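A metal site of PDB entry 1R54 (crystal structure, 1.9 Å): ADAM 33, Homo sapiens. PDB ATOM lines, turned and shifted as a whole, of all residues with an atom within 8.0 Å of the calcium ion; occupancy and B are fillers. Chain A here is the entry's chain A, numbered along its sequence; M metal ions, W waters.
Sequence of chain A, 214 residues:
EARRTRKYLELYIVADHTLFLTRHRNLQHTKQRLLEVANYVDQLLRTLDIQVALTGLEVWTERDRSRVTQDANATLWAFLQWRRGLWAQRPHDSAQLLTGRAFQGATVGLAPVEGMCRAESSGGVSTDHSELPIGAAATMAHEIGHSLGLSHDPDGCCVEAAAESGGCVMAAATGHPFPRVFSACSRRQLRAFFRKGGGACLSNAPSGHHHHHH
O of Glu 10 sits at hydrogen-bond distance from N of Ser 94, at 3.2 Å. SG of Cys 201 is disulfide-bonded to SG of Cys 117, 2.0 Å away.
The backbone carbonyl oxygen (O) of Cys 201 binds the calcium ion (2.3 Å). OE1 of Glu 10 binds the calcium ion, at 2.3 Å. OD1 of Asn 204 is bound to the calcium ion (2.4 Å). The calcium ion is bound by water W1 (2.4 Å). OD1 of Asp 93 is bound to the calcium ion. OD2 of Asp 93 binds the calcium ion (2.5 Å).
Water W1 bridges O of Tyr 8 (2.6 Å) and O of Asn 204 (2.8 Å).
Four residues have an atom within 4 Å of the calcium ion: Glu 10, Asp 93, Cys 201 and Asn 204.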
ATOM      1  N   TYR A   8      12.200  -6.739   5.063  1.00  0.00           N
ATOM      2  CA  TYR A   8      12.332  -6.659   3.616  1.00  0.00           C
ATOM      3  C   TYR A   8      11.169  -5.899   2.998  1.00  0.00           C
ATOM      4  O   TYR A   8      10.004  -6.188   3.284  1.00  0.00           O
ATOM      5  CB  TYR A   8      12.394  -8.050   2.994  1.00  0.00           C
ATOM      6  CG  TYR A   8      13.380  -8.979   3.669  1.00  0.00           C
ATOM      7  CD1 TYR A   8      13.080  -9.566   4.899  1.00  0.00           C
ATOM      8  CD2 TYR A   8      14.605  -9.268   3.076  1.00  0.00           C
ATOM      9  CE1 TYR A   8      13.984 -10.405   5.533  1.00  0.00           C
ATOM     10  CE2 TYR A   8      15.526 -10.121   3.708  1.00  0.00           C
ATOM     11  CZ  TYR A   8      15.199 -10.677   4.930  1.00  0.00           C
ATOM     12  OH  TYR A   8      16.102 -11.509   5.556  1.00  0.00           O
ATOM     13  N   LEU A   9      11.496  -4.922   2.162  1.00  0.00           N
ATOM     14  CA  LEU A   9      10.481  -4.145   1.479  1.00  0.00           C
ATOM     15  C   LEU A   9      10.432  -4.606   0.030  1.00  0.00           C
ATOM     16  O   LEU A   9      11.363  -4.366  -0.743  1.00  0.00           O
ATOM     17  CB  LEU A   9      10.816  -2.650   1.503  1.00  0.00           C
ATOM     18  CG  LEU A   9       9.800  -1.799   0.739  1.00  0.00           C
ATOM     19  CD1 LEU A   9       8.467  -1.814   1.485  1.00  0.00           C
ATOM     20  CD2 LEU A   9      10.318  -0.372   0.576  1.00  0.00           C
ATOM     21  N   GLU A  10       9.354  -5.297  -0.337  1.00  0.00           N
ATOM     22  CA  GLU A  10       9.177  -5.756  -1.707  1.00  0.00           C
ATOM     23  C   GLU A  10       8.657  -4.554  -2.465  1.00  0.00           C
ATOM     24  O   GLU A  10       7.508  -4.122  -2.298  1.00  0.00           O
ATOM     25  CB  GLU A  10       8.199  -6.925  -1.734  1.00  0.00           C
ATOM     26  CG  GLU A  10       8.787  -8.152  -1.051  1.00  0.00           C
ATOM     27  CD  GLU A  10       7.815  -9.309  -0.974  1.00  0.00           C
ATOM     28  OE1 GLU A  10       6.872  -9.244  -0.157  1.00  0.00           O
ATOM     29  OE2 GLU A  10       8.003 -10.296  -1.718  1.00  0.00           O
ATOM     30  N   LEU A  11       9.530  -4.004  -3.291  1.00  0.00           N
ATOM     31  CA  LEU A  11       9.261  -2.793  -4.044  1.00  0.00           C
ATOM     32  C   LEU A  11       8.973  -2.974  -5.526  1.00  0.00           C
ATOM     33  O   LEU A  11       9.663  -3.716  -6.210  1.00  0.00           O
ATOM     34  CB  LEU A  11      10.473  -1.870  -3.872  1.00  0.00           C
ATOM     35  CG  LEU A  11      10.519  -0.489  -4.518  1.00  0.00           C
ATOM     36  CD1 LEU A  11       9.575   0.462  -3.793  1.00  0.00           C
ATOM     37  CD2 LEU A  11      11.956   0.025  -4.438  1.00  0.00           C
ATOM     38  N   ALA A  53      13.808  -5.453  -1.879  1.00  0.00           N
ATOM     39  CA  ALA A  53      13.692  -6.601  -2.780  1.00  0.00           C
ATOM     40  C   ALA A  53      12.858  -6.063  -3.948  1.00  0.00           C
ATOM     41  O   ALA A  53      11.662  -5.804  -3.804  1.00  0.00           O
ATOM     42  CB  ALA A  53      12.969  -7.740  -2.084  1.00  0.00           C
ATOM     43  N   THR A  55      10.614  -6.287  -6.631  1.00  0.00           N
ATOM     44  CA  THR A  55       9.607  -7.213  -7.151  1.00  0.00           C
ATOM     45  C   THR A  55       9.400  -7.052  -8.655  1.00  0.00           C
ATOM     46  O   THR A  55       9.350  -8.042  -9.388  1.00  0.00           O
ATOM     47  CB  THR A  55       8.236  -6.987  -6.454  1.00  0.00           C
ATOM     48  OG1 THR A  55       8.383  -7.177  -5.046  1.00  0.00           O
ATOM     49  CG2 THR A  55       7.186  -7.954  -6.989  1.00  0.00           C
ATOM     50  N   PRO A  91       2.001  -9.065  -6.694  1.00  0.00           N
ATOM     51  CA  PRO A  91       2.069  -8.673  -5.282  1.00  0.00           C
ATOM     52  C   PRO A  91       3.376  -7.978  -4.939  1.00  0.00           C
ATOM     53  O   PRO A  91       4.438  -8.349  -5.441  1.00  0.00           O
ATOM     54  CB  PRO A  91       1.907 -10.002  -4.557  1.00  0.00           C
ATOM     55  CG  PRO A  91       1.057 -10.796  -5.486  1.00  0.00           C
ATOM     56  CD  PRO A  91       1.682 -10.497  -6.826  1.00  0.00           C
ATOM     57  N   HIS A  92       3.288  -6.977  -4.065  1.00  0.00           N
ATOM     58  CA  HIS A  92       4.446  -6.208  -3.629  1.00  0.00           C
ATOM     59  C   HIS A  92       4.000  -5.458  -2.390  1.00  0.00           C
ATOM     60  O   HIS A  92       2.805  -5.356  -2.115  1.00  0.00           O
ATOM     61  CB  HIS A  92       4.860  -5.216  -4.710  1.00  0.00           C
ATOM     62  CG  HIS A  92       3.768  -4.274  -5.112  1.00  0.00           C
ATOM     63  ND1 HIS A  92       2.809  -4.602  -6.054  1.00  0.00           N
ATOM     64  CD2 HIS A  92       3.425  -3.051  -4.644  1.00  0.00           C
ATOM     65  CE1 HIS A  92       1.938  -3.628  -6.144  1.00  0.00           C
ATOM     66  NE2 HIS A  92       2.282  -2.668  -5.301  1.00  0.00           N
ATOM     67  N   ASP A  93       4.952  -4.914  -1.632  1.00  0.00           N
ATOM     68  CA  ASP A  93       4.608  -4.177  -0.422  1.00  0.00           C
ATOM     69  C   ASP A  93       4.311  -2.709  -0.700  1.00  0.00           C
ATOM     70  O   ASP A  93       3.351  -2.145  -0.167  1.00  0.00           O
ATOM     71  CB  ASP A  93       5.731  -4.267   0.607  1.00  0.00           C
ATOM     72  CG  ASP A  93       5.992  -5.682   1.074  1.00  0.00           C
ATOM     73  OD1 ASP A  93       5.023  -6.468   1.169  1.00  0.00           O
ATOM     74  OD2 ASP A  93       7.162  -6.003   1.351  1.00  0.00           O
ATOM     75  N   SER A  94       5.128  -2.090  -1.549  1.00  0.00           N
ATOM     76  CA  SER A  94       4.978  -0.677  -1.876  1.00  0.00           C
ATOM     77  C   SER A  94       5.286  -0.424  -3.362  1.00  0.00           C
ATOM     78  O   SER A  94       6.231  -0.983  -3.902  1.00  0.00           O
ATOM     79  CB  SER A  94       5.931   0.141  -0.984  1.00  0.00           C
ATOM     80  OG  SER A  94       5.865   1.527  -1.255  1.00  0.00           O
ATOM     81  N   CYS A 117       1.751  -1.023   3.436  1.00  0.00           N
ATOM     82  CA  CYS A 117       1.054  -2.307   3.420  1.00  0.00           C
ATOM     83  C   CYS A 117      -0.468  -2.219   3.214  1.00  0.00           C
ATOM     84  O   CYS A 117      -1.105  -3.230   2.931  1.00  0.00           O
ATOM     85  CB  CYS A 117       1.324  -3.099   4.706  1.00  0.00           C
ATOM     86  SG  CYS A 117       3.072  -3.459   5.103  1.00  0.00           S
ATOM     87  N   GLY A 199       3.324  -1.844   9.353  1.00  0.00           N
ATOM     88  CA  GLY A 199       4.204  -2.471   8.388  1.00  0.00           C
ATOM     89  C   GLY A 199       4.348  -3.978   8.511  1.00  0.00           C
ATOM     90  O   GLY A 199       5.433  -4.530   8.317  1.00  0.00           O
ATOM     91  N   ALA A 200       3.245  -4.645   8.830  1.00  0.00           N
ATOM     92  CA  ALA A 200       3.249  -6.094   8.989  1.00  0.00           C
ATOM     93  C   ALA A 200       3.765  -6.831   7.748  1.00  0.00           C
ATOM     94  O   ALA A 200       4.394  -7.887   7.861  1.00  0.00           O
ATOM     95  CB  ALA A 200       1.841  -6.582   9.330  1.00  0.00           C
ATOM     96  N   CYS A 201       3.529  -6.259   6.572  1.00  0.00           N
ATOM     97  CA  CYS A 201       3.939  -6.927   5.330  1.00  0.00           C
ATOM     98  C   CYS A 201       5.436  -6.953   5.030  1.00  0.00           C
ATOM     99  O   CYS A 201       5.850  -7.587   4.059  1.00  0.00           O
ATOM    100  CB  CYS A 201       3.188  -6.334   4.128  1.00  0.00           C
ATOM    101  SG  CYS A 201       3.693  -4.669   3.586  1.00  0.00           S
ATOM    102  N   LEU A 202       6.260  -6.297   5.841  1.00  0.00           N
ATOM    103  CA  LEU A 202       7.705  -6.312   5.614  1.00  0.00           C
ATOM    104  C   LEU A 202       8.390  -7.477   6.321  1.00  0.00           C
ATOM    105  O   LEU A 202       9.613  -7.553   6.361  1.00  0.00           O
ATOM    106  CB  LEU A 202       8.353  -5.000   6.067  1.00  0.00           C
ATOM    107  CG  LEU A 202       8.113  -3.759   5.214  1.00  0.00           C
ATOM    108  CD1 LEU A 202       6.742  -3.172   5.516  1.00  0.00           C
ATOM    109  CD2 LEU A 202       9.190  -2.722   5.509  1.00  0.00           C
ATOM    110  N   SER A 203       7.595  -8.388   6.881  1.00  0.00           N
ATOM    111  CA  SER A 203       8.145  -9.522   7.612  1.00  0.00           C
ATOM    112  C   SER A 203       8.697 -10.662   6.776  1.00  0.00           C
ATOM    113  O   SER A 203       9.645 -11.325   7.195  1.00  0.00           O
ATOM    114  CB  SER A 203       7.095 -10.079   8.571  1.00  0.00           C
ATOM    115  OG  SER A 203       6.814  -9.149   9.604  1.00  0.00           O
ATOM    116  N   ASN A 204       8.111 -10.919   5.616  1.00  0.00           N
ATOM    117  CA  ASN A 204       8.574 -12.036   4.802  1.00  0.00           C
ATOM    118  C   ASN A 204       9.814 -11.764   3.989  1.00  0.00           C
ATOM    119  O   ASN A 204       9.983 -10.692   3.399  1.00  0.00           O
ATOM    120  CB  ASN A 204       7.459 -12.529   3.862  1.00  0.00           C
ATOM    121  CG  ASN A 204       7.097 -11.504   2.800  1.00  0.00           C
ATOM    122  OD1 ASN A 204       6.627 -10.415   3.105  1.00  0.00           O
ATOM    123  ND2 ASN A 204       7.308 -11.874   1.533  1.00  0.00           N
ATOM    124  N   ALA A 205      10.708 -12.745   3.974  1.00  0.00           N
ATOM    125  CA  ALA A 205      11.929 -12.634   3.197  1.00  0.00           C
ATOM    126  C   ALA A 205      11.545 -13.109   1.795  1.00  0.00           C
ATOM    127  O   ALA A 205      10.957 -14.179   1.639  1.00  0.00           O
ATOM    128  CB  ALA A 205      13.011 -13.547   3.788  1.00  0.00           C
ATOM    129  N   PRO A 206      11.845 -12.309   0.766  1.00  0.00           N
ATOM    130  CA  PRO A 206      11.493 -12.718  -0.597  1.00  0.00           C
ATOM    131  C   PRO A 206      12.177 -14.002  -1.059  1.00  0.00           C
ATOM    132  O   PRO A 206      11.540 -14.767  -1.811  1.00  0.00           O
ATOM    133  CB  PRO A 206      11.866 -11.490  -1.435  1.00  0.00           C
ATOM    134  CG  PRO A 206      12.961 -10.859  -0.639  1.00  0.00           C
ATOM    135  CD  PRO A 206      12.453 -10.970   0.779  1.00  0.00           C
HETATM  136 CA    CA M   1       6.414  -8.335   1.952  1.00  0.00          CA
HETATM  137  O   HOH W   1       8.778  -8.360   2.564  1.00  0.00           O
